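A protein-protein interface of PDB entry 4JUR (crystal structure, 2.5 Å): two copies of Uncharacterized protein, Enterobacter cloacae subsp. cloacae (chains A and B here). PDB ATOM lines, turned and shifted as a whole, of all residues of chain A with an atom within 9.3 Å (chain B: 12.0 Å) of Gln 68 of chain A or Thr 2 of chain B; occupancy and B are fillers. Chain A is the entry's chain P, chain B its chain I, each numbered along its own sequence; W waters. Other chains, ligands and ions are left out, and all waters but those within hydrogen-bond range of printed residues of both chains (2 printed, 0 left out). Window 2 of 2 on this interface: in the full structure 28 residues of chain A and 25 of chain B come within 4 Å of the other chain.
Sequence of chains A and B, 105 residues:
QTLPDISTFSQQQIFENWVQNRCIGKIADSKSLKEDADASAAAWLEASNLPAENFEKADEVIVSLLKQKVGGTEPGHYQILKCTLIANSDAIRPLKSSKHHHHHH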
ATOM      1  N   VAL A  61     -23.719  23.959   6.440  1.00  0.00           N
ATOM      2  CA  VAL A  61     -22.596  23.149   5.950  1.00  0.00           C
ATOM      3  C   VAL A  61     -21.247  23.817   6.211  1.00  0.00           C
ATOM      4  O   VAL A  61     -20.279  23.144   6.555  1.00  0.00           O
ATOM      5  CB  VAL A  61     -22.719  22.805   4.442  1.00  0.00           C
ATOM      6  CG1 VAL A  61     -21.501  22.041   3.961  1.00  0.00           C
ATOM      7  CG2 VAL A  61     -23.999  22.016   4.174  1.00  0.00           C
ATOM      8  N   ILE A  62     -21.179  25.136   6.073  1.00  0.00           N
ATOM      9  CA  ILE A  62     -19.939  25.841   6.377  1.00  0.00           C
ATOM     10  C   ILE A  62     -19.543  25.638   7.837  1.00  0.00           C
ATOM     11  O   ILE A  62     -18.375  25.341   8.134  1.00  0.00           O
ATOM     12  CB  ILE A  62     -20.064  27.348   6.105  1.00  0.00           C
ATOM     13  CG1 ILE A  62     -20.133  27.619   4.605  1.00  0.00           C
ATOM     14  CG2 ILE A  62     -18.912  28.115   6.734  1.00  0.00           C
ATOM     15  CD1 ILE A  62     -20.726  28.971   4.287  1.00  0.00           C
ATOM     16  N   VAL A  63     -20.512  25.791   8.744  1.00  0.00           N
ATOM     17  CA  VAL A  63     -20.232  25.672  10.179  1.00  0.00           C
ATOM     18  C   VAL A  63     -19.694  24.278  10.471  1.00  0.00           C
ATOM     19  O   VAL A  63     -18.679  24.107  11.153  1.00  0.00           O
ATOM     20  CB  VAL A  63     -21.489  25.935  11.062  1.00  0.00           C
ATOM     21  CG1 VAL A  63     -21.130  25.812  12.549  1.00  0.00           C
ATOM     22  CG2 VAL A  63     -22.124  27.319  10.758  1.00  0.00           C
ATOM     23  N   SER A  64     -20.372  23.281   9.918  1.00  0.00           N
ATOM     24  CA  SER A  64     -19.922  21.900  10.058  1.00  0.00           C
ATOM     25  C   SER A  64     -18.503  21.623   9.502  1.00  0.00           C
ATOM     26  O   SER A  64     -17.652  21.035  10.181  1.00  0.00           O
ATOM     27  CB  SER A  64     -20.932  20.953   9.401  1.00  0.00           C
ATOM     28  OG  SER A  64     -20.679  19.620   9.797  1.00  0.00           O
ATOM     29  N   LEU A  65     -18.248  22.038   8.269  1.00  0.00           N
ATOM     30  CA  LEU A  65     -16.987  21.700   7.629  1.00  0.00           C
ATOM     31  C   LEU A  65     -15.816  22.489   8.203  1.00  0.00           C
ATOM     32  O   LEU A  65     -14.669  22.084   8.047  1.00  0.00           O
ATOM     33  CB  LEU A  65     -17.067  21.891   6.114  1.00  0.00           C
ATOM     34  CG  LEU A  65     -17.898  20.894   5.307  1.00  0.00           C
ATOM     35  CD1 LEU A  65     -17.728  21.151   3.818  1.00  0.00           C
ATOM     36  CD2 LEU A  65     -17.497  19.474   5.640  1.00  0.00           C
ATOM     37  N   LEU A  66     -16.089  23.604   8.872  1.00  0.00           N
ATOM     38  CA  LEU A  66     -14.995  24.384   9.441  1.00  0.00           C
ATOM     39  C   LEU A  66     -14.314  23.665  10.600  1.00  0.00           C
ATOM     40  O   LEU A  66     -13.179  23.982  10.949  1.00  0.00           O
ATOM     41  CB  LEU A  66     -15.473  25.762   9.890  1.00  0.00           C
ATOM     42  CG  LEU A  66     -15.371  26.876   8.858  1.00  0.00           C
ATOM     43  CD1 LEU A  66     -15.763  28.184   9.487  1.00  0.00           C
ATOM     44  CD2 LEU A  66     -13.974  26.944   8.340  1.00  0.00           C
ATOM     45  N   LYS A  67     -15.008  22.703  11.201  1.00  0.00           N
ATOM     46  CA  LYS A  67     -14.451  21.947  12.328  1.00  0.00           C
ATOM     47  C   LYS A  67     -13.321  21.038  11.862  1.00  0.00           C
ATOM     48  O   LYS A  67     -12.367  20.797  12.598  1.00  0.00           O
ATOM     49  CB  LYS A  67     -15.529  21.112  13.021  1.00  0.00           C
ATOM     50  CG  LYS A  67     -16.660  21.915  13.666  1.00  0.00           C
ATOM     51  CD  LYS A  67     -17.556  21.001  14.498  1.00  0.00           C
ATOM     52  CE  LYS A  67     -18.976  21.546  14.603  1.00  0.00           C
ATOM     53  NZ  LYS A  67     -19.013  22.982  15.080  1.00  0.00           N
ATOM     54  N   GLN A  68     -13.459  20.538  10.635  1.00  0.00           N
ATOM     55  CA  GLN A  68     -12.472  19.703   9.950  1.00  0.00           C
ATOM     56  C   GLN A  68     -11.077  20.295  10.031  1.00  0.00           C
ATOM     57  O   GLN A  68     -10.911  21.507   9.895  1.00  0.00           O
ATOM     58  CB  GLN A  68     -12.868  19.607   8.478  1.00  0.00           C
ATOM     59  CG  GLN A  68     -12.190  18.534   7.687  1.00  0.00           C
ATOM     60  CD  GLN A  68     -13.154  17.423   7.320  1.00  0.00           C
ATOM     61  OE1 GLN A  68     -14.327  17.446   7.708  1.00  0.00           O
ATOM     62  NE2 GLN A  68     -12.662  16.439   6.566  1.00  0.00           N
ATOM     63  N   LYS A  69     -10.071  19.450  10.241  1.00  0.00           N
ATOM     64  CA  LYS A  69      -8.692  19.937  10.339  1.00  0.00           C
ATOM     65  C   LYS A  69      -7.964  19.897   8.983  1.00  0.00           C
ATOM     66  O   LYS A  69      -7.978  18.874   8.304  1.00  0.00           O
ATOM     67  CB  LYS A  69      -7.910  19.144  11.390  1.00  0.00           C
ATOM     68  N   VAL A  70      -7.350  21.015   8.594  1.00  0.00           N
ATOM     69  CA  VAL A  70      -6.532  21.065   7.379  1.00  0.00           C
ATOM     70  C   VAL A  70      -5.110  21.444   7.754  1.00  0.00           C
ATOM     71  O   VAL A  70      -4.850  22.569   8.171  1.00  0.00           O
ATOM     72  CB  VAL A  70      -7.079  22.067   6.335  1.00  0.00           C
ATOM     73  CG1 VAL A  70      -6.110  22.225   5.188  1.00  0.00           C
ATOM     74  CG2 VAL A  70      -8.411  21.603   5.818  1.00  0.00           C
ATOM     75  N   GLY A  71      -4.191  20.491   7.620  1.00  0.00           N
ATOM     76  CA  GLY A  71      -2.822  20.688   8.060  1.00  0.00           C
ATOM     77  C   GLY A  71      -1.840  20.903   6.923  1.00  0.00           C
ATOM     78  O   GLY A  71      -2.226  20.978   5.748  1.00  0.00           O
ATOM     79  N   HIS A  77      -3.497  26.735  11.028  1.00  0.00           N
ATOM     80  CA  HIS A  77      -4.692  25.908  10.829  1.00  0.00           C
ATOM     81  C   HIS A  77      -5.246  25.919   9.409  1.00  0.00           C
ATOM     82  O   HIS A  77      -6.235  25.224   9.147  1.00  0.00           O
ATOM     83  CB  HIS A  77      -5.817  26.312  11.791  1.00  0.00           C
ATOM     84  CG  HIS A  77      -5.424  26.258  13.232  1.00  0.00           C
ATOM     85  ND1 HIS A  77      -4.256  25.665  13.662  1.00  0.00           N
ATOM     86  CD2 HIS A  77      -6.036  26.740  14.339  1.00  0.00           C
ATOM     87  CE1 HIS A  77      -4.164  25.781  14.978  1.00  0.00           C
ATOM     88  NE2 HIS A  77      -5.235  26.423  15.410  1.00  0.00           N
ATOM     89  N   TYR A  78      -4.631  26.723   8.528  1.00  0.00           N
ATOM     90  CA  TYR A  78      -4.959  26.775   7.095  1.00  0.00           C
ATOM     91  C   TYR A  78      -6.416  27.119   6.806  1.00  0.00           C
ATOM     92  O   TYR A  78      -7.032  26.541   5.909  1.00  0.00           O
ATOM     93  CB  TYR A  78      -4.631  25.441   6.417  1.00  0.00           C
ATOM     94  CG  TYR A  78      -3.164  25.235   6.167  1.00  0.00           C
ATOM     95  CD1 TYR A  78      -2.575  25.697   5.003  1.00  0.00           C
ATOM     96  CD2 TYR A  78      -2.358  24.587   7.100  1.00  0.00           C
ATOM     97  CE1 TYR A  78      -1.242  25.526   4.770  1.00  0.00           C
ATOM     98  CE2 TYR A  78      -1.018  24.409   6.867  1.00  0.00           C
ATOM     99  CZ  TYR A  78      -0.470  24.879   5.706  1.00  0.00           C
ATOM    100  OH  TYR A  78       0.854  24.703   5.451  1.00  0.00           O
ATOM    101  N   GLN A  79      -6.968  28.052   7.562  1.00  0.00           N
ATOM    102  CA  GLN A  79      -8.384  28.337   7.451  1.00  0.00           C
ATOM    103  C   GLN A  79      -8.709  28.978   6.110  1.00  0.00           C
ATOM    104  O   GLN A  79      -9.747  28.676   5.536  1.00  0.00           O
ATOM    105  CB  GLN A  79      -8.832  29.237   8.599  1.00  0.00           C
ATOM    106  CG  GLN A  79      -8.474  28.705   9.965  1.00  0.00           C
ATOM    107  CD  GLN A  79      -9.670  28.122  10.704  1.00  0.00           C
ATOM    108  OE1 GLN A  79     -10.243  27.097  10.309  1.00  0.00           O
ATOM    109  NE2 GLN A  79     -10.057  28.785  11.791  1.00  0.00           N
ATOM    110  N   LYS A  82      -8.839  26.398   3.709  1.00  0.00           N
ATOM    111  CA  LYS A  82     -10.002  25.601   4.059  1.00  0.00           C
ATOM    112  C   LYS A  82     -11.318  26.208   3.528  1.00  0.00           C
ATOM    113  O   LYS A  82     -12.213  25.480   3.124  1.00  0.00           O
ATOM    114  CB  LYS A  82     -10.047  25.352   5.567  1.00  0.00           C
ATOM    115  CG  LYS A  82     -11.045  24.283   5.974  1.00  0.00           C
ATOM    116  CD  LYS A  82     -11.416  24.425   7.428  1.00  0.00           C
ATOM    117  CE  LYS A  82     -10.192  24.298   8.306  1.00  0.00           C
ATOM    118  NZ  LYS A  82     -10.469  24.690   9.718  1.00  0.00           N
ATOM    119  N   CYS A  83     -11.422  27.533   3.505  1.00  0.00           N
ATOM    120  CA  CYS A  83     -12.623  28.216   2.990  1.00  0.00           C
ATOM    121  C   CYS A  83     -12.882  27.972   1.515  1.00  0.00           C
ATOM    122  O   CYS A  83     -14.006  27.647   1.135  1.00  0.00           O
ATOM    123  CB  CYS A  83     -12.552  29.721   3.240  1.00  0.00           C
ATOM    124  SG  CYS A  83     -12.906  30.170   4.949  1.00  0.00           S
ATOM    125  N   LEU A  85     -11.742  25.417  -0.071  1.00  0.00           N
ATOM    126  CA  LEU A  85     -12.058  24.001  -0.223  1.00  0.00           C
ATOM    127  C   LEU A  85     -13.522  23.768   0.071  1.00  0.00           C
ATOM    128  O   LEU A  85     -14.209  22.985  -0.605  1.00  0.00           O
ATOM    129  CB  LEU A  85     -11.190  23.137   0.680  1.00  0.00           C
ATOM    130  CG  LEU A  85      -9.722  23.299   0.299  1.00  0.00           C
ATOM    131  CD1 LEU A  85      -8.832  22.393   1.121  1.00  0.00           C
ATOM    132  CD2 LEU A  85      -9.535  23.063  -1.186  1.00  0.00           C
ATOM    133  N   ILE A  86     -13.997  24.452   1.097  1.00  0.00           N
ATOM    134  CA  ILE A  86     -15.374  24.299   1.525  1.00  0.00           C
ATOM    135  C   ILE A  86     -16.335  24.748   0.409  1.00  0.00           C
ATOM    136  O   ILE A  86     -17.338  24.074   0.126  1.00  0.00           O
ATOM    137  CB  ILE A  86     -15.598  25.059   2.834  1.00  0.00           C
ATOM    138  CG1 ILE A  86     -15.006  24.253   3.985  1.00  0.00           C
ATOM    139  CG2 ILE A  86     -17.056  25.322   3.062  1.00  0.00           C
ATOM    140  CD1 ILE A  86     -15.007  24.995   5.311  1.00  0.00           C
ATOM    141  N   ALA A  87     -15.998  25.859  -0.243  1.00  0.00           N
ATOM    142  CA  ALA A  87     -16.819  26.378  -1.333  1.00  0.00           C
ATOM    143  C   ALA A  87     -16.911  25.414  -2.522  1.00  0.00           C
ATOM    144  O   ALA A  87     -17.840  25.501  -3.340  1.00  0.00           O
ATOM    145  CB  ALA A  87     -16.287  27.710  -1.787  1.00  0.00           C
ATOM    146  N   ASN A  88     -15.941  24.508  -2.628  1.00  0.00           N
ATOM    147  CA  ASN A  88     -15.872  23.581  -3.756  1.00  0.00           C
ATOM    148  C   ASN A  88     -16.128  22.139  -3.318  1.00  0.00           C
ATOM    149  O   ASN A  88     -15.895  21.212  -4.077  1.00  0.00           O
ATOM    150  CB  ASN A  88     -14.525  23.697  -4.507  1.00  0.00           C
ATOM    151  CG  ASN A  88     -14.327  25.060  -5.184  1.00  0.00           C
ATOM    152  OD1 ASN A  88     -14.763  25.272  -6.318  1.00  0.00           O
ATOM    153  ND2 ASN A  88     -13.666  25.984  -4.489  1.00  0.00           N
ATOM    154  N   SER A  89     -16.621  21.962  -2.096  1.00  0.00           N
ATOM    155  CA  SER A  89     -16.894  20.632  -1.541  1.00  0.00           C
ATOM    156  C   SER A  89     -18.147  19.915  -2.063  1.00  0.00           C
ATOM    157  O   SER A  89     -19.112  20.546  -2.486  1.00  0.00           O
ATOM    158  CB  SER A  89     -17.001  20.713  -0.015  1.00  0.00           C
ATOM    159  OG  SER A  89     -18.153  21.443   0.367  1.00  0.00           O
ATOM    160  N   ASP A  90     -18.111  18.589  -1.994  1.00  0.00           N
ATOM    161  CA  ASP A  90     -19.256  17.717  -2.259  1.00  0.00           C
ATOM    162  C   ASP A  90     -20.513  18.142  -1.496  1.00  0.00           C
ATOM    163  O   ASP A  90     -21.617  18.121  -2.028  1.00  0.00           O
ATOM    164  CB  ASP A  90     -18.924  16.276  -1.818  1.00  0.00           C
ATOM    165  CG  ASP A  90     -17.959  15.556  -2.765  1.00  0.00           C
ATOM    166  OD1 ASP A  90     -17.635  16.113  -3.842  1.00  0.00           O
ATOM    167  OD2 ASP A  90     -17.549  14.413  -2.433  1.00  0.00           O
ATOM    168  N   ALA A  91     -20.327  18.497  -0.231  1.00  0.00           N
ATOM    169  CA  ALA A  91     -21.420  18.804   0.681  1.00  0.00           C
ATOM    170  C   ALA A  91     -22.184  20.070   0.289  1.00  0.00           C
ATOM    171  O   ALA A  91     -23.392  20.180   0.534  1.00  0.00           O
ATOM    172  CB  ALA A  91     -20.875  18.921   2.109  1.00  0.00           C
ATOM    173  N   ILE A  92     -21.463  21.019  -0.310  1.00  0.00           N
ATOM    174  CA  ILE A  92     -22.055  22.251  -0.819  1.00  0.00           C
ATOM    175  C   ILE A  92     -22.723  22.113  -2.200  1.00  0.00           C
ATOM    176  O   ILE A  92     -23.714  22.773  -2.468  1.00  0.00           O
ATOM    177  CB  ILE A  92     -21.012  23.380  -0.832  1.00  0.00           C
ATOM    178  CG1 ILE A  92     -20.823  23.945   0.575  1.00  0.00           C
ATOM    179  CG2 ILE A  92     -21.392  24.488  -1.795  1.00  0.00           C
ATOM    180  CD1 ILE A  92     -22.013  24.765   1.109  1.00  0.00           C
ATOM    181  N   ARG A  93     -22.197  21.248  -3.067  1.00  0.00           N
ATOM    182  CA  ARG A  93     -22.722  21.114  -4.433  1.00  0.00           C
ATOM    183  C   ARG A  93     -24.254  20.996  -4.629  1.00  0.00           C
ATOM    184  O   ARG A  93     -24.811  21.709  -5.477  1.00  0.00           O
ATOM    185  CB  ARG A  93     -21.993  20.012  -5.219  1.00  0.00           C
ATOM    186  CG  ARG A  93     -20.893  20.581  -6.099  1.00  0.00           C
ATOM    187  CD  ARG A  93     -20.662  19.790  -7.384  1.00  0.00           C
ATOM    188  NE  ARG A  93     -20.228  18.433  -7.088  1.00  0.00           N
ATOM    189  CZ  ARG A  93     -19.019  18.121  -6.636  1.00  0.00           C
ATOM    190  NH1 ARG A  93     -18.109  19.069  -6.418  1.00  0.00           N
ATOM    191  NH2 ARG A  93     -18.727  16.852  -6.392  1.00  0.00           N
ATOM    192  N   THR B   2     -13.396  14.449   3.219  1.00  0.00           N
ATOM    193  CA  THR B   2     -14.623  15.221   2.997  1.00  0.00           C
ATOM    194  C   THR B   2     -14.392  16.633   2.401  1.00  0.00           C
ATOM    195  O   THR B   2     -15.340  17.284   1.971  1.00  0.00           O
ATOM    196  CB  THR B   2     -15.511  15.285   4.283  1.00  0.00           C
ATOM    197  OG1 THR B   2     -16.883  15.005   3.955  1.00  0.00           O
ATOM    198  CG2 THR B   2     -15.436  16.647   4.941  1.00  0.00           C
ATOM    199  N   LEU B   3     -13.144  17.105   2.377  1.00  0.00           N
ATOM    200  CA  LEU B   3     -12.776  18.250   1.526  1.00  0.00           C
ATOM    201  C   LEU B   3     -12.007  17.762   0.282  1.00  0.00           C
ATOM    202  O   LEU B   3     -11.298  16.756   0.338  1.00  0.00           O
ATOM    203  CB  LEU B   3     -11.947  19.297   2.290  1.00  0.00           C
ATOM    204  CG  LEU B   3     -12.572  19.993   3.505  1.00  0.00           C
ATOM    205  CD1 LEU B   3     -11.557  20.864   4.191  1.00  0.00           C
ATOM    206  CD2 LEU B   3     -13.758  20.825   3.128  1.00  0.00           C
ATOM    207  N   PRO B   4     -12.144  18.466  -0.852  1.00  0.00           N
ATOM    208  CA  PRO B   4     -11.380  18.041  -2.030  1.00  0.00           C
ATOM    209  C   PRO B   4      -9.899  18.369  -1.919  1.00  0.00           C
ATOM    210  O   PRO B   4      -9.528  19.396  -1.352  1.00  0.00           O
ATOM    211  CB  PRO B   4     -11.988  18.869  -3.158  1.00  0.00           C
ATOM    212  CG  PRO B   4     -12.558  20.067  -2.478  1.00  0.00           C
ATOM    213  CD  PRO B   4     -13.061  19.579  -1.157  1.00  0.00           C
ATOM    214  N   ASP B   5      -9.065  17.493  -2.472  1.00  0.00           N
ATOM    215  CA  ASP B   5      -7.653  17.767  -2.595  1.00  0.00           C
ATOM    216  C   ASP B   5      -7.454  18.925  -3.553  1.00  0.00           C
ATOM    217  O   ASP B   5      -8.248  19.141  -4.476  1.00  0.00           O
ATOM    218  CB  ASP B   5      -6.897  16.541  -3.106  1.00  0.00           C
ATOM    219  CG  ASP B   5      -6.415  15.623  -1.980  1.00  0.00           C
ATOM    220  OD1 ASP B   5      -6.498  16.023  -0.786  1.00  0.00           O
ATOM    221  OD2 ASP B   5      -5.938  14.499  -2.296  1.00  0.00           O
ATOM    222  N   ILE B   6      -6.377  19.660  -3.324  1.00  0.00           N
ATOM    223  CA  ILE B   6      -5.981  20.747  -4.194  1.00  0.00           C
ATOM    224  C   ILE B   6      -5.785  20.297  -5.636  1.00  0.00           C
ATOM    225  O   ILE B   6      -6.189  20.995  -6.577  1.00  0.00           O
ATOM    226  CB  ILE B   6      -4.695  21.373  -3.677  1.00  0.00           C
ATOM    227  CG1 ILE B   6      -5.018  22.213  -2.455  1.00  0.00           C
ATOM    228  CG2 ILE B   6      -4.058  22.255  -4.728  1.00  0.00           C
ATOM    229  CD1 ILE B   6      -3.811  22.878  -1.861  1.00  0.00           C
ATOM    230  N   THR B   8      -7.280  18.421  -7.549  1.00  0.00           N
ATOM    231  CA  THR B   8      -8.491  18.235  -8.359  1.00  0.00           C
ATOM    232  C   THR B   8      -9.067  19.513  -8.939  1.00  0.00           C
ATOM    233  O   THR B   8     -10.101  19.454  -9.601  1.00  0.00           O
ATOM    234  CB  THR B   8      -9.647  17.517  -7.588  1.00  0.00           C
ATOM    235  OG1 THR B   8     -10.272  18.437  -6.678  1.00  0.00           O
ATOM    236  CG2 THR B   8      -9.139  16.289  -6.829  1.00  0.00           C
ATOM    237  N   PHE B   9      -8.424  20.651  -8.669  1.00  0.00           N
ATOM    238  CA  PHE B   9      -8.753  21.944  -9.303  1.00  0.00           C
ATOM    239  C   PHE B   9      -8.006  22.041 -10.643  1.00  0.00           C
ATOM    240  O   PHE B   9      -6.986  21.397 -10.809  1.00  0.00           O
ATOM    241  CB  PHE B   9      -8.316  23.139  -8.399  1.00  0.00           C
ATOM    242  CG  PHE B   9      -9.150  23.327  -7.154  1.00  0.00           C
ATOM    243  CD1 PHE B   9     -10.010  24.417  -7.037  1.00  0.00           C
ATOM    244  CD2 PHE B   9      -9.076  22.422  -6.099  1.00  0.00           C
ATOM    245  CE1 PHE B   9     -10.803  24.595  -5.906  1.00  0.00           C
ATOM    246  CE2 PHE B   9      -9.863  22.587  -4.948  1.00  0.00           C
ATOM    247  CZ  PHE B   9     -10.735  23.670  -4.855  1.00  0.00           C
ATOM    248  N   ASP B  36      -1.694  32.572   8.135  1.00  0.00           N
ATOM    249  CA  ASP B  36      -2.620  31.584   7.593  1.00  0.00           C
ATOM    250  C   ASP B  36      -2.792  31.764   6.078  1.00  0.00           C
ATOM    251  O   ASP B  36      -2.766  30.797   5.310  1.00  0.00           O
ATOM    252  CB  ASP B  36      -3.967  31.709   8.303  1.00  0.00           C
ATOM    253  CG  ASP B  36      -4.954  30.626   7.895  1.00  0.00           C
ATOM    254  OD1 ASP B  36      -5.593  30.031   8.797  1.00  0.00           O
ATOM    255  OD2 ASP B  36      -5.123  30.382   6.683  1.00  0.00           O
ATOM    256  N   SER B  40      -1.537  29.160   3.207  1.00  0.00           N
ATOM    257  CA  SER B  40      -2.574  28.748   2.273  1.00  0.00           C
ATOM    258  C   SER B  40      -2.134  28.982   0.828  1.00  0.00           C
ATOM    259  O   SER B  40      -2.209  28.070   0.005  1.00  0.00           O
ATOM    260  CB  SER B  40      -3.889  29.461   2.569  1.00  0.00           C
ATOM    261  OG  SER B  40      -4.439  28.980   3.786  1.00  0.00           O
HETATM  262  O   HOH W   1     -17.903  17.562   1.068  1.00  0.00           O
HETATM  263  O   HOH W   2     -15.853  17.428  -1.359  1.00  0.00           O
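OD1 of Asp 36 of chain B sits at hydrogen-bond distance from N of Tyr 78 of chain A (3.5 Å). The side-chain carboxylate of Asp 36 of chain B is in hydrogen-bond range of the backbone NH of Gln 79 of chain A (2.7 Å).
Water W2 lies within hydrogen-bond range of N of Asp 90 of chain A (2.6 Å) and O of Thr 2 of chain B (3.4 Å). Water W1 lies within hydrogen-bond range of O of Thr 2 of chain B (2.7 Å), N of Ala 91 of chain A (2.9 Å) and N of Asp 90 of chain A (3.2 Å).
No position is printed for both chains.
Among the printed residues, pairs that only touch across the chains: Gln 68 of chain A with Thr 2 of chain B, Asn 88 of chain A with Phe 9 of chain B, Leu 65 of chain A with Thr 2 of chain B, Val 70 of chain A with Leu 3 of chain B, Leu 85 of chain A with Pro 4 of chain B, Ile 86 of chain A with Leu 3 of chain B, Leu 85 of chain A with Phe 9 of chain B, Asn 88 of chain A with Pro 4 of chain B, Lys 82 of chain A with Leu 3 of chain B, Tyr 78 of chain A with Ser 40 of chain B and Ser 89 of chain A with Pro 4 of chain B.
Of chain B, only Thr 2 comes within 4 Å of Leu 65 of chain A. No residue of chain B comes within 4 Å of Lys 67 of chain A. Printed residues of chain B within 4 Å of Gln 68 of chain A: Thr 2 (3.1 Å). Lys 69 of chain A touches none of the printed residues of chain B. Of the printed residues of chain B, Val 70 of chain A touches Leu 3 (3.6 Å). Of the printed residues of chain B, Lys 82 of chain A touches Leu 3 (3.9 Å). Of the printed residues of chain B, Leu 85 of chain A touches Pro 4 and Phe 9. Printed residues of chain B within 4 Å of Ile 86 of chain A: Leu 3 (3.7 Å). No residue of chain B comes within 4 Å of Asp 90 of chain A. Ile 92 of chain A touches none of the printed residues of chain B. Printed residues of chain A within 4 Å of Pro 4 of chain B: Leu 85 (3.6 Å), Asn 88 (3.9 Å) and Ser 89 (3.99 Å). Of the printed residues of chain A, Asp 36 of chain B touches Tyr 78 (3.5 Å) and Gln 79 (2.7 Å).
Of the 25 printed residues of chain A, 10 touch a printed residue of chain B. Hydrophobic or aromatic side chains of chain A that line the printed part of chain B: Leu 65, Val 70, Tyr 78, Leu 85 and Ile 86. Printed residues of chain B that touch a printed residue of chain A: Thr 2, Leu 3, Pro 4, Phe 9, Asp 36 and Ser 40. Among the printed residues, no Asp or Glu carboxylate lies within 4 Å of a Lys or Arg side-chain nitrogen of the other chain.
OG of Ser 40 of chain B lies within hydrogen-bond range of O of Asp 36 of chain B. NZ of Lys 82 of chain A sits at hydrogen-bond distance from O of Leu 66 of chain A, 3.1 Å away. The backbone carbonyl oxygen (O) of Gln 68 of chain A sits at hydrogen-bond distance from the side-chain amino group (NZ) of Lys 82 of chain A. The side-chain amino group (NZ) of Lys 82 of chain A sits at hydrogen-bond distance from the side-chain amide oxygen (OE1) of Gln 79 of chain A. OG of Ser 89 of chain A sits at hydrogen-bond distance from O of Ile 86 of chain A (2.8 Å). OG of Ser 89 of chain A lies within hydrogen-bond range of N of Ile 92 of chain A, 3.4 Å away.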
